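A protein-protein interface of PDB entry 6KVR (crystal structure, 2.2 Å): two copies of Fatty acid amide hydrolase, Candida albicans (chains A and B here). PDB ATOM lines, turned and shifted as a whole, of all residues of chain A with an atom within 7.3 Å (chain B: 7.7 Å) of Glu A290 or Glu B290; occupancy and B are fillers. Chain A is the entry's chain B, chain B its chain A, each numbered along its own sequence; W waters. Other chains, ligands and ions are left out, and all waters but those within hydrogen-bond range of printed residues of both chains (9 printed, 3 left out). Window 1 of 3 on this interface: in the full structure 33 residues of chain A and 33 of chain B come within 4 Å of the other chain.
Gly A288 touches Arg B438, and with the chains exchanged Arg A438 touches Gly B288. Gly A288 touches Asn B441, and with the chains exchanged Asn A441 touches Gly B288. Glu A290 touches Asn B441, and with the chains exchanged Asn A441 touches Glu B290. Met A395 touches Arg B438, and with the chains exchanged Arg A438 touches Met B395.
The side-chain carboxylate (OE2) of Glu A290 is in salt-bridge range of the guanidinium group (NH2) of Arg B444. O of Gly A288 sits at hydrogen-bond distance from ND2 of Asn B441. O of Gly B288 is in hydrogen-bond range of ND2 of Asn A441 (2.9 Å). The side-chain carboxylate (OE2) of Glu B290 is in salt-bridge range of the guanidinium group (NH2) of Arg A444, at 2.9 Å.
Of chain B, only Glu B290 (3.7 Å), Asn B441 (3.6 Å) and Arg B444 (2.7 Å) come within 4 Å of Glu A290. Of the printed residues of chain A, Glu B290 touches Glu A290 (3.7 Å), Asn A441 (3.5 Å) and Arg A444 (2.9 Å). Of the printed residues of chain B, Gly A288 touches Arg B438 (3.5 Å), Asn B441 (2.8 Å) and Val B442 (3.7 Å). Of the printed residues of chain B, Ala A287 touches Arg B438 (3.8 Å) and Val B442 (3.9 Å). Of the printed residues of chain A, Met B395 touches Arg A438 (3.7 Å). Ser A291 touches none of the printed residues of chain B. Asn A437 touches none of the printed residues of chain B. The nearest printed residue of chain B that does not touch Gly A288 is Asn B437 (5.5 Å).
Water W9 lies within hydrogen-bond range of the side-chain carboxylate (OE2) of Glu B290 (2.5 Å), the backbone carbonyl oxygen (O) of Glu A290 (2.9 Å) and the guanidinium group (NH1) of Arg A444 (3.2 Å). Water W8 lies within hydrogen-bond range of the side-chain amide oxygen (OE1) of Gln B289 (2.9 Å), the backbone carbonyl oxygen (O) of Met B395 (2.9 Å) and the guanidinium group (NH2) of Arg A438 (3.3 Å). Water W5 lies within hydrogen-bond range of O of Ala A287 and NH1 of Arg B438. Water W1 bridges the side-chain hydroxyl (OG1) of Thr B325 (3.2 Å) and the backbone carbonyl oxygen (O) of Asp A445 (3.5 Å).
OD1 of Asp B445 is in salt-bridge range of NE of Arg B444. The side-chain amide oxygen (OE1) of Gln B289 is in hydrogen-bond range of the backbone NH (N) of Ser B291, at 2.9 Å. The side-chain hydroxyl (OG) of Ser A291 is in hydrogen-bond range of the side-chain amide oxygen (OD1) of Asn A441 (2.9 Å). The side-chain hydroxyl (OG) of Ser B291 sits at hydrogen-bond distance from the side-chain amide oxygen (OD1) of Asn B441 (2.7 Å). N of Ser A291 is in hydrogen-bond range of OE1 of Gln A289, 2.8 Å away. The side-chain carboxylate of Asp A445 lies within salt-bridge range of the guanidinium group of Arg A444, 3.0 Å away.
Among the printed residues, pairs that only touch across the chains: Arg A438 with Gly B288 (3.3 Å), Arg A438 with Gln B289 (3.5 Å), Gly A288 with Arg B438 (3.5 Å), Asn A441 with Glu B290 (3.5 Å), Gln A289 with Arg B438 (3.5 Å), Glu A290 with Asn B441 (3.6 Å), Lys A275 with Lys B275 (3.7 Å), Gly A288 with Val B442 (3.7 Å), Glu A290 with Glu B290 (3.7 Å), Arg A438 with Met B395 (3.7 Å), Ala A287 with Arg B438 (3.8 Å), Arg A438 with Ala B287 (3.8 Å), Met A395 with Arg B438 (3.9 Å) and Ala A287 with Val B442 (3.9 Å).
Of the 18 printed residues of chain A, 9 touch a printed residue of chain B. Printed residues of chain A that touch a printed residue of chain B: Lys A275, Ala A287, Gly A288, Gln A289, Glu A290, Met A395, Arg A438, Asn A441 and Arg A444. Of the 20 printed residues of chain B, 10 touch a printed residue of chain A. Printed residues of chain B that touch a printed residue of chain A: Lys B275, Ala B287, Gly B288, Gln B289, Glu B290, Met B395, Arg B438, Asn B441, Val B442 and Arg B444. Hydrophobic or aromatic side chains of chain B that line the printed part of chain A: Val B442. Among the printed residues, Asp or Glu carboxylates within 4 Å of a Lys or Arg side-chain nitrogen of the other chain: Glu A290 with Arg B444 (2.7 Å) and Arg A444 with Glu B290 (2.9 Å).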
ATOM      1  N   LYS A 275       2.393  29.090 -17.654  1.00  0.00           N
ATOM      2  CA  LYS A 275       2.450  28.630 -19.041  1.00  0.00           C
ATOM      3  C   LYS A 275       1.115  28.109 -19.563  1.00  0.00           C
ATOM      4  O   LYS A 275       1.061  27.549 -20.670  1.00  0.00           O
ATOM      5  CB  LYS A 275       3.560  27.588 -19.226  1.00  0.00           C
ATOM      6  CG  LYS A 275       4.914  28.281 -19.345  1.00  0.00           C
ATOM      7  CD  LYS A 275       6.043  27.564 -18.639  1.00  0.00           C
ATOM      8  CE  LYS A 275       7.306  28.459 -18.675  1.00  0.00           C
ATOM      9  NZ  LYS A 275       8.267  28.197 -17.553  1.00  0.00           N
ATOM     10  N   GLY A 286      10.226  42.495 -16.667  1.00  0.00           N
ATOM     11  CA  GLY A 286      10.487  41.066 -16.561  1.00  0.00           C
ATOM     12  C   GLY A 286      10.921  40.333 -17.820  1.00  0.00           C
ATOM     13  O   GLY A 286      10.811  39.101 -17.884  1.00  0.00           O
ATOM     14  N   ALA A 287      11.420  41.047 -18.824  1.00  0.00           N
ATOM     15  CA  ALA A 287      11.797  40.379 -20.072  1.00  0.00           C
ATOM     16  C   ALA A 287      12.911  39.379 -19.809  1.00  0.00           C
ATOM     17  O   ALA A 287      13.961  39.740 -19.275  1.00  0.00           O
ATOM     18  CB  ALA A 287      12.241  41.395 -21.125  1.00  0.00           C
ATOM     19  N   GLY A 288      12.675  38.115 -20.180  1.00  0.00           N
ATOM     20  CA  GLY A 288      13.666  37.070 -20.015  1.00  0.00           C
ATOM     21  C   GLY A 288      13.779  36.481 -18.624  1.00  0.00           C
ATOM     22  O   GLY A 288      14.575  35.556 -18.428  1.00  0.00           O
ATOM     23  N   GLN A 289      13.025  36.977 -17.651  1.00  0.00           N
ATOM     24  CA  GLN A 289      13.092  36.455 -16.293  1.00  0.00           C
ATOM     25  C   GLN A 289      12.259  35.174 -16.210  1.00  0.00           C
ATOM     26  O   GLN A 289      11.060  35.178 -16.506  1.00  0.00           O
ATOM     27  CB  GLN A 289      12.613  37.536 -15.317  1.00  0.00           C
ATOM     28  CG  GLN A 289      12.828  37.321 -13.801  1.00  0.00           C
ATOM     29  CD  GLN A 289      11.988  36.195 -13.203  1.00  0.00           C
ATOM     30  OE1 GLN A 289      12.516  35.159 -12.782  1.00  0.00           O
ATOM     31  NE2 GLN A 289      10.677  36.362 -13.236  1.00  0.00           N
ATOM     32  N   GLU A 290      12.902  34.076 -15.820  1.00  0.00           N
ATOM     33  CA  GLU A 290      12.313  32.740 -15.824  1.00  0.00           C
ATOM     34  C   GLU A 290      12.339  32.026 -14.480  1.00  0.00           C
ATOM     35  O   GLU A 290      11.698  30.977 -14.353  1.00  0.00           O
ATOM     36  CB  GLU A 290      13.066  31.831 -16.803  1.00  0.00           C
ATOM     37  CG  GLU A 290      12.776  32.022 -18.236  1.00  0.00           C
ATOM     38  CD  GLU A 290      13.193  30.787 -18.997  1.00  0.00           C
ATOM     39  OE1 GLU A 290      14.409  30.457 -18.956  1.00  0.00           O
ATOM     40  OE2 GLU A 290      12.306  30.140 -19.607  1.00  0.00           O
ATOM     41  N   SER A 291      13.114  32.507 -13.511  1.00  0.00           N
ATOM     42  CA  SER A 291      13.232  31.806 -12.233  1.00  0.00           C
ATOM     43  C   SER A 291      11.882  31.700 -11.520  1.00  0.00           C
ATOM     44  O   SER A 291      11.518  30.622 -11.037  1.00  0.00           O
ATOM     45  CB  SER A 291      14.256  32.521 -11.357  1.00  0.00           C
ATOM     46  OG  SER A 291      15.537  32.442 -11.960  1.00  0.00           O
ATOM     47  N   VAL A 292      11.160  32.823 -11.404  1.00  0.00           N
ATOM     48  CA  VAL A 292       9.775  32.924 -10.916  1.00  0.00           C
ATOM     49  C   VAL A 292       8.943  33.538 -12.026  1.00  0.00           C
ATOM     50  O   VAL A 292       8.810  34.777 -12.074  1.00  0.00           O
ATOM     51  CB  VAL A 292       9.613  33.822  -9.676  1.00  0.00           C
ATOM     52  CG1 VAL A 292       8.226  33.625  -9.058  1.00  0.00           C
ATOM     53  CG2 VAL A 292      10.582  33.510  -8.679  1.00  0.00           C
ATOM     54  N   PRO A 293       8.393  32.742 -12.936  1.00  0.00           N
ATOM     55  CA  PRO A 293       7.660  33.325 -14.060  1.00  0.00           C
ATOM     56  C   PRO A 293       6.368  33.957 -13.569  1.00  0.00           C
ATOM     57  O   PRO A 293       5.674  33.412 -12.706  1.00  0.00           O
ATOM     58  CB  PRO A 293       7.395  32.128 -14.991  1.00  0.00           C
ATOM     59  CG  PRO A 293       8.248  30.992 -14.465  1.00  0.00           C
ATOM     60  CD  PRO A 293       8.470  31.269 -13.006  1.00  0.00           C
ATOM     61  N   ALA A 294       6.099  35.152 -14.086  1.00  0.00           N
ATOM     62  CA  ALA A 294       4.813  35.807 -13.927  1.00  0.00           C
ATOM     63  C   ALA A 294       3.713  35.031 -14.646  1.00  0.00           C
ATOM     64  O   ALA A 294       3.948  34.258 -15.586  1.00  0.00           O
ATOM     65  CB  ALA A 294       4.869  37.234 -14.469  1.00  0.00           C
ATOM     66  N   THR A 325       5.292  29.724 -25.923  1.00  0.00           N
ATOM     67  CA  THR A 325       5.499  29.425 -24.508  1.00  0.00           C
ATOM     68  C   THR A 325       4.282  28.744 -23.872  1.00  0.00           C
ATOM     69  O   THR A 325       4.436  27.930 -22.946  1.00  0.00           O
ATOM     70  CB  THR A 325       5.840  30.731 -23.781  1.00  0.00           C
ATOM     71  OG1 THR A 325       7.166  31.129 -24.139  1.00  0.00           O
ATOM     72  CG2 THR A 325       5.746  30.591 -22.260  1.00  0.00           C
ATOM     73  N   MET A 395      15.336  36.300  -6.124  1.00  0.00           N
ATOM     74  CA  MET A 395      15.026  36.210  -7.551  1.00  0.00           C
ATOM     75  C   MET A 395      14.438  37.502  -8.106  1.00  0.00           C
ATOM     76  O   MET A 395      14.730  37.856  -9.237  1.00  0.00           O
ATOM     77  CB  MET A 395      14.062  35.057  -7.845  1.00  0.00           C
ATOM     78  CG  MET A 395      14.611  33.676  -7.471  1.00  0.00           C
ATOM     79  SD  MET A 395      13.258  32.270  -7.682  1.00  0.00           S
ATOM     80  CE  MET A 395      14.481  30.761  -8.061  1.00  0.00           C
ATOM     81  N   ASN A 437      22.403  32.632  -9.850  1.00  0.00           N
ATOM     82  CA  ASN A 437      20.993  32.527 -10.232  1.00  0.00           C
ATOM     83  C   ASN A 437      20.598  31.064 -10.394  1.00  0.00           C
ATOM     84  O   ASN A 437      19.504  30.666  -9.984  1.00  0.00           O
ATOM     85  CB  ASN A 437      20.758  33.325 -11.515  1.00  0.00           C
ATOM     86  CG  ASN A 437      19.259  33.554 -11.854  1.00  0.00           C
ATOM     87  OD1 ASN A 437      18.958  34.380 -12.718  1.00  0.00           O
ATOM     88  ND2 ASN A 437      18.341  32.826 -11.208  1.00  0.00           N
ATOM     89  N   ARG A 438      21.508  30.239 -10.945  1.00  0.00           N
ATOM     90  CA  ARG A 438      21.253  28.806 -11.071  1.00  0.00           C
ATOM     91  C   ARG A 438      21.108  28.127  -9.713  1.00  0.00           C
ATOM     92  O   ARG A 438      20.325  27.181  -9.582  1.00  0.00           O
ATOM     93  CB  ARG A 438      22.369  28.135 -11.872  1.00  0.00           C
ATOM     94  CG  ARG A 438      22.295  28.414 -13.351  1.00  0.00           C
ATOM     95  CD  ARG A 438      23.234  27.530 -14.154  1.00  0.00           C
ATOM     96  NE  ARG A 438      23.428  28.022 -15.516  1.00  0.00           N
ATOM     97  CZ  ARG A 438      24.368  27.569 -16.340  1.00  0.00           C
ATOM     98  NH1 ARG A 438      25.164  26.561 -15.997  1.00  0.00           N
ATOM     99  NH2 ARG A 438      24.528  28.152 -17.528  1.00  0.00           N
ATOM    100  N   ASN A 441      17.585  28.635  -8.682  1.00  0.00           N
ATOM    101  CA  ASN A 441      16.736  27.674  -9.391  1.00  0.00           C
ATOM    102  C   ASN A 441      16.780  26.307  -8.719  1.00  0.00           C
ATOM    103  O   ASN A 441      15.741  25.651  -8.558  1.00  0.00           O
ATOM    104  CB  ASN A 441      17.168  27.542 -10.864  1.00  0.00           C
ATOM    105  CG  ASN A 441      16.931  28.824 -11.683  1.00  0.00           C
ATOM    106  OD1 ASN A 441      16.076  29.637 -11.345  1.00  0.00           O
ATOM    107  ND2 ASN A 441      17.698  28.998 -12.766  1.00  0.00           N
ATOM    108  N   ARG A 444      14.670  26.527  -5.581  1.00  0.00           N
ATOM    109  CA  ARG A 444      13.266  26.508  -6.000  1.00  0.00           C
ATOM    110  C   ARG A 444      12.775  25.088  -6.268  1.00  0.00           C
ATOM    111  O   ARG A 444      11.664  24.716  -5.867  1.00  0.00           O
ATOM    112  CB  ARG A 444      13.086  27.364  -7.255  1.00  0.00           C
ATOM    113  CG  ARG A 444      11.678  27.336  -7.834  1.00  0.00           C
ATOM    114  CD  ARG A 444      11.657  27.803  -9.293  1.00  0.00           C
ATOM    115  NE  ARG A 444      12.377  26.854 -10.128  1.00  0.00           N
ATOM    116  CZ  ARG A 444      12.802  27.093 -11.360  1.00  0.00           C
ATOM    117  NH1 ARG A 444      12.594  28.258 -11.953  1.00  0.00           N
ATOM    118  NH2 ARG A 444      13.446  26.136 -12.019  1.00  0.00           N
ATOM    119  N   ASP A 445      13.586  24.277  -6.955  1.00  0.00           N
ATOM    120  CA  ASP A 445      13.127  22.940  -7.318  1.00  0.00           C
ATOM    121  C   ASP A 445      13.129  21.995  -6.120  1.00  0.00           C
ATOM    122  O   ASP A 445      12.262  21.118  -6.037  1.00  0.00           O
ATOM    123  CB  ASP A 445      13.973  22.394  -8.470  1.00  0.00           C
ATOM    124  CG  ASP A 445      13.669  23.107  -9.811  1.00  0.00           C
ATOM    125  OD1 ASP A 445      12.668  23.863  -9.913  1.00  0.00           O
ATOM    126  OD2 ASP A 445      14.470  22.957 -10.753  1.00  0.00           O
ATOM    127  N   ARG A 448       9.806  22.912  -4.382  1.00  0.00           N
ATOM    128  CA  ARG A 448       8.650  22.377  -5.098  1.00  0.00           C
ATOM    129  C   ARG A 448       8.463  20.898  -4.811  1.00  0.00           C
ATOM    130  O   ARG A 448       7.351  20.442  -4.520  1.00  0.00           O
ATOM    131  CB  ARG A 448       8.802  22.612  -6.595  1.00  0.00           C
ATOM    132  CG  ARG A 448       8.497  24.030  -6.999  1.00  0.00           C
ATOM    133  CD  ARG A 448       8.646  24.216  -8.493  1.00  0.00           C
ATOM    134  NE  ARG A 448       8.592  25.633  -8.811  1.00  0.00           N
ATOM    135  CZ  ARG A 448       8.605  26.124 -10.040  1.00  0.00           C
ATOM    136  NH1 ARG A 448       8.746  25.340 -11.094  1.00  0.00           N
ATOM    137  NH2 ARG A 448       8.453  27.434 -10.214  1.00  0.00           N
ATOM    138  N   THR B 274      10.580  19.357 -23.753  1.00  0.00           N
ATOM    139  CA  THR B 274      11.020  19.391 -22.363  1.00  0.00           C
ATOM    140  C   THR B 274       9.846  19.191 -21.415  1.00  0.00           C
ATOM    141  O   THR B 274       8.695  19.524 -21.726  1.00  0.00           O
ATOM    142  CB  THR B 274      11.718  20.708 -22.019  1.00  0.00           C
ATOM    143  OG1 THR B 274      10.852  21.806 -22.341  1.00  0.00           O
ATOM    144  CG2 THR B 274      13.048  20.854 -22.780  1.00  0.00           C
ATOM    145  N   LYS B 275      10.159  18.627 -20.249  1.00  0.00           N
ATOM    146  CA  LYS B 275       9.283  18.519 -19.086  1.00  0.00           C
ATOM    147  C   LYS B 275       8.201  17.460 -19.236  1.00  0.00           C
ATOM    148  O   LYS B 275       7.220  17.480 -18.509  1.00  0.00           O
ATOM    149  CB  LYS B 275       8.665  19.873 -18.724  1.00  0.00           C
ATOM    150  CG  LYS B 275       9.724  20.974 -18.544  1.00  0.00           C
ATOM    151  CD  LYS B 275       9.296  22.281 -19.209  1.00  0.00           C
ATOM    152  CE  LYS B 275       8.749  23.307 -18.183  1.00  0.00           C
ATOM    153  NZ  LYS B 275       7.877  24.397 -18.771  1.00  0.00           N
ATOM    154  N   GLY B 286      24.728  20.580 -15.116  1.00  0.00           N
ATOM    155  CA  GLY B 286      23.581  21.396 -15.467  1.00  0.00           C
ATOM    156  C   GLY B 286      22.644  21.812 -14.352  1.00  0.00           C
ATOM    157  O   GLY B 286      21.548  22.311 -14.646  1.00  0.00           O
ATOM    158  N   ALA B 287      23.033  21.643 -13.083  1.00  0.00           N
ATOM    159  CA  ALA B 287      22.143  21.986 -11.974  1.00  0.00           C
ATOM    160  C   ALA B 287      21.725  23.454 -12.048  1.00  0.00           C
ATOM    161  O   ALA B 287      22.570  24.351 -12.081  1.00  0.00           O
ATOM    162  CB  ALA B 287      22.826  21.701 -10.634  1.00  0.00           C
ATOM    163  N   GLY B 288      20.415  23.694 -12.081  1.00  0.00           N
ATOM    164  CA  GLY B 288      19.889  25.037 -12.107  1.00  0.00           C
ATOM    165  C   GLY B 288      19.837  25.665 -13.480  1.00  0.00           C
ATOM    166  O   GLY B 288      19.389  26.817 -13.600  1.00  0.00           O
ATOM    167  N   GLN B 289      20.293  24.963 -14.517  1.00  0.00           N
ATOM    168  CA  GLN B 289      20.389  25.540 -15.851  1.00  0.00           C
ATOM    169  C   GLN B 289      19.049  25.348 -16.572  1.00  0.00           C
ATOM    170  O   GLN B 289      18.583  24.220 -16.757  1.00  0.00           O
ATOM    171  CB  GLN B 289      21.565  24.913 -16.603  1.00  0.00           C
ATOM    172  CG  GLN B 289      22.024  25.574 -17.914  1.00  0.00           C
ATOM    173  CD  GLN B 289      21.002  25.470 -19.025  1.00  0.00           C
ATOM    174  OE1 GLN B 289      20.483  26.479 -19.506  1.00  0.00           O
ATOM    175  NE2 GLN B 289      20.682  24.244 -19.415  1.00  0.00           N
ATOM    176  N   GLU B 290      18.446  26.459 -16.990  1.00  0.00           N
ATOM    177  CA  GLU B 290      17.078  26.486 -17.471  1.00  0.00           C
ATOM    178  C   GLU B 290      16.926  27.154 -18.829  1.00  0.00           C
ATOM    179  O   GLU B 290      15.837  27.080 -19.415  1.00  0.00           O
ATOM    180  CB  GLU B 290      16.205  27.248 -16.463  1.00  0.00           C
ATOM    181  CG  GLU B 290      15.457  26.416 -15.481  1.00  0.00           C
ATOM    182  CD  GLU B 290      14.350  27.226 -14.834  1.00  0.00           C
ATOM    183  OE1 GLU B 290      14.639  28.361 -14.361  1.00  0.00           O
ATOM    184  OE2 GLU B 290      13.193  26.744 -14.829  1.00  0.00           O
ATOM    185  N   SER B 291      17.947  27.857 -19.314  1.00  0.00           N
ATOM    186  CA  SER B 291      17.812  28.564 -20.585  1.00  0.00           C
ATOM    187  C   SER B 291      17.655  27.590 -21.750  1.00  0.00           C
ATOM    188  O   SER B 291      16.855  27.835 -22.663  1.00  0.00           O
ATOM    189  CB  SER B 291      19.003  29.497 -20.794  1.00  0.00           C
ATOM    190  OG  SER B 291      18.931  30.618 -19.898  1.00  0.00           O
ATOM    191  N   VAL B 292      18.400  26.486 -21.742  1.00  0.00           N
ATOM    192  CA  VAL B 292      18.183  25.402 -22.698  1.00  0.00           C
ATOM    193  C   VAL B 292      18.189  24.099 -21.907  1.00  0.00           C
ATOM    194  O   VAL B 292      19.242  23.459 -21.733  1.00  0.00           O
ATOM    195  CB  VAL B 292      19.213  25.423 -23.847  1.00  0.00           C
ATOM    196  CG1 VAL B 292      20.668  25.472 -23.345  1.00  0.00           C
ATOM    197  CG2 VAL B 292      18.991  24.242 -24.777  1.00  0.00           C
ATOM    198  N   PRO B 293      17.044  23.688 -21.374  1.00  0.00           N
ATOM    199  CA  PRO B 293      17.035  22.528 -20.479  1.00  0.00           C
ATOM    200  C   PRO B 293      17.261  21.226 -21.234  1.00  0.00           C
ATOM    201  O   PRO B 293      16.823  21.052 -22.373  1.00  0.00           O
ATOM    202  CB  PRO B 293      15.640  22.577 -19.834  1.00  0.00           C
ATOM    203  CG  PRO B 293      14.809  23.405 -20.742  1.00  0.00           C
ATOM    204  CD  PRO B 293      15.737  24.366 -21.438  1.00  0.00           C
ATOM    205  N   ALA B 294      17.977  20.320 -20.578  1.00  0.00           N
ATOM    206  CA  ALA B 294      18.197  18.983 -21.083  1.00  0.00           C
ATOM    207  C   ALA B 294      16.891  18.192 -21.068  1.00  0.00           C
ATOM    208  O   ALA B 294      15.874  18.610 -20.514  1.00  0.00           O
ATOM    209  CB  ALA B 294      19.254  18.266 -20.249  1.00  0.00           C
ATOM    210  N   THR B 325       8.732  19.113 -11.603  1.00  0.00           N
ATOM    211  CA  THR B 325       8.970  19.716 -12.915  1.00  0.00           C
ATOM    212  C   THR B 325       8.208  18.997 -14.027  1.00  0.00           C
ATOM    213  O   THR B 325       7.890  19.607 -15.059  1.00  0.00           O
ATOM    214  CB  THR B 325      10.471  19.689 -13.225  1.00  0.00           C
ATOM    215  OG1 THR B 325      11.187  20.366 -12.188  1.00  0.00           O
ATOM    216  CG2 THR B 325      10.775  20.353 -14.567  1.00  0.00           C
ATOM    217  N   MET B 395      24.727  29.934 -24.310  1.00  0.00           N
ATOM    218  CA  MET B 395      23.923  29.445 -23.186  1.00  0.00           C
ATOM    219  C   MET B 395      24.629  28.292 -22.501  1.00  0.00           C
ATOM    220  O   MET B 395      24.580  28.169 -21.277  1.00  0.00           O
ATOM    221  CB  MET B 395      22.531  28.978 -23.640  1.00  0.00           C
ATOM    222  CG  MET B 395      21.473  30.070 -23.793  1.00  0.00           C
ATOM    223  SD  MET B 395      19.801  29.349 -24.590  1.00  0.00           S
ATOM    224  CE  MET B 395      18.614  30.862 -24.307  1.00  0.00           C
ATOM    225  N   ASN B 437      22.099  37.007 -19.276  1.00  0.00           N
ATOM    226  CA  ASN B 437      21.461  35.705 -19.470  1.00  0.00           C
ATOM    227  C   ASN B 437      19.998  35.871 -19.874  1.00  0.00           C
ATOM    228  O   ASN B 437      19.508  35.158 -20.756  1.00  0.00           O
ATOM    229  CB  ASN B 437      21.582  34.862 -18.193  1.00  0.00           C
ATOM    230  CG  ASN B 437      21.278  33.366 -18.423  1.00  0.00           C
ATOM    231  OD1 ASN B 437      20.783  32.959 -19.473  1.00  0.00           O
ATOM    232  ND2 ASN B 437      21.563  32.553 -17.418  1.00  0.00           N
ATOM    233  N   ARG B 438      19.296  36.834 -19.261  1.00  0.00           N
ATOM    234  CA  ARG B 438      17.897  37.077 -19.605  1.00  0.00           C
ATOM    235  C   ARG B 438      17.728  37.520 -21.058  1.00  0.00           C
ATOM    236  O   ARG B 438      16.747  37.137 -21.713  1.00  0.00           O
ATOM    237  CB  ARG B 438      17.303  38.117 -18.654  1.00  0.00           C
ATOM    238  CG  ARG B 438      17.109  37.597 -17.254  1.00  0.00           C
ATOM    239  CD  ARG B 438      16.298  38.579 -16.424  1.00  0.00           C
ATOM    240  NE  ARG B 438      16.339  38.234 -15.012  1.00  0.00           N
ATOM    241  CZ  ARG B 438      15.919  39.035 -14.046  1.00  0.00           C
ATOM    242  NH1 ARG B 438      15.382  40.211 -14.318  1.00  0.00           N
ATOM    243  NH2 ARG B 438      16.049  38.647 -12.778  1.00  0.00           N
ATOM    244  N   ASN B 441      17.577  34.539 -23.181  1.00  0.00           N
ATOM    245  CA  ASN B 441      16.231  33.980 -23.061  1.00  0.00           C
ATOM    246  C   ASN B 441      15.250  34.678 -23.998  1.00  0.00           C
ATOM    247  O   ASN B 441      14.357  34.033 -24.567  1.00  0.00           O
ATOM    248  CB  ASN B 441      15.721  34.122 -21.616  1.00  0.00           C
ATOM    249  CG  ASN B 441      16.444  33.225 -20.632  1.00  0.00           C
ATOM    250  OD1 ASN B 441      17.116  32.252 -21.016  1.00  0.00           O
ATOM    251  ND2 ASN B 441      16.309  33.543 -19.344  1.00  0.00           N
ATOM    252  N   VAL B 442      15.357  36.007 -24.108  1.00  0.00           N
ATOM    253  CA  VAL B 442      14.480  36.777 -24.991  1.00  0.00           C
ATOM    254  C   VAL B 442      14.683  36.344 -26.438  1.00  0.00           C
ATOM    255  O   VAL B 442      13.719  36.095 -27.170  1.00  0.00           O
ATOM    256  CB  VAL B 442      14.723  38.292 -24.819  1.00  0.00           C
ATOM    257  CG1 VAL B 442      14.069  39.080 -25.964  1.00  0.00           C
ATOM    258  CG2 VAL B 442      14.184  38.791 -23.469  1.00  0.00           C
ATOM    259  N   ARG B 444      15.786  33.458 -27.471  1.00  0.00           N
ATOM    260  CA  ARG B 444      15.216  32.118 -27.594  1.00  0.00           C
ATOM    261  C   ARG B 444      13.711  32.177 -27.821  1.00  0.00           C
ATOM    262  O   ARG B 444      13.162  31.443 -28.652  1.00  0.00           O
ATOM    263  CB  ARG B 444      15.523  31.310 -26.332  1.00  0.00           C
ATOM    264  CG  ARG B 444      14.868  29.946 -26.275  1.00  0.00           C
ATOM    265  CD  ARG B 444      14.851  29.431 -24.846  1.00  0.00           C
ATOM    266  NE  ARG B 444      13.935  30.222 -24.036  1.00  0.00           N
ATOM    267  CZ  ARG B 444      13.858  30.198 -22.710  1.00  0.00           C
ATOM    268  NH1 ARG B 444      14.623  29.402 -21.982  1.00  0.00           N
ATOM    269  NH2 ARG B 444      12.982  30.994 -22.100  1.00  0.00           N
ATOM    270  N   ASP B 445      13.021  33.022 -27.069  1.00  0.00           N
ATOM    271  CA  ASP B 445      11.577  33.089 -27.211  1.00  0.00           C
ATOM    272  C   ASP B 445      11.188  33.650 -28.572  1.00  0.00           C
ATOM    273  O   ASP B 445      10.211  33.189 -29.180  1.00  0.00           O
ATOM    274  CB  ASP B 445      10.987  33.910 -26.069  1.00  0.00           C
ATOM    275  CG  ASP B 445      11.068  33.176 -24.734  1.00  0.00           C
ATOM    276  OD1 ASP B 445      11.398  31.954 -24.736  1.00  0.00           O
ATOM    277  OD2 ASP B 445      10.776  33.805 -23.689  1.00  0.00           O
ATOM    278  N   ARG B 448      11.648  30.798 -31.098  1.00  0.00           N
ATOM    279  CA  ARG B 448      10.571  29.829 -30.951  1.00  0.00           C
ATOM    280  C   ARG B 448       9.283  30.316 -31.609  1.00  0.00           C
ATOM    281  O   ARG B 448       8.582  29.536 -32.269  1.00  0.00           O
ATOM    282  CB  ARG B 448      10.331  29.536 -29.472  1.00  0.00           C
ATOM    283  CG  ARG B 448      11.359  28.597 -28.882  1.00  0.00           C
ATOM    284  CD  ARG B 448      11.140  28.396 -27.387  1.00  0.00           C
ATOM    285  NE  ARG B 448      12.223  27.603 -26.815  1.00  0.00           N
ATOM    286  CZ  ARG B 448      12.225  27.112 -25.582  1.00  0.00           C
ATOM    287  NH1 ARG B 448      11.244  27.380 -24.732  1.00  0.00           N
ATOM    288  NH2 ARG B 448      13.233  26.328 -25.197  1.00  0.00           N
HETATM  289  O   HOH W   1      10.610  20.506  -9.050  1.00  0.00           O
HETATM  290  O   HOH W   2      16.720  35.697 -13.478  1.00  0.00           O
HETATM  291  O   HOH W   3      22.042  29.815 -17.457  1.00  0.00           O
HETATM  292  O   HOH W   4      14.866  35.912 -11.206  1.00  0.00           O
HETATM  293  O   HOH W   5      14.328  41.533 -16.930  1.00  0.00           O
HETATM  294  O   HOH W   6      13.111  27.538 -19.732  1.00  0.00           O
HETATM  295  O   HOH W   7      25.022  24.567 -13.526  1.00  0.00           O
HETATM  296  O   HOH W   8      22.174  28.792 -19.810  1.00  0.00           O
HETATM  297  O   HOH W   9      11.194  28.177 -14.820  1.00  0.00           O
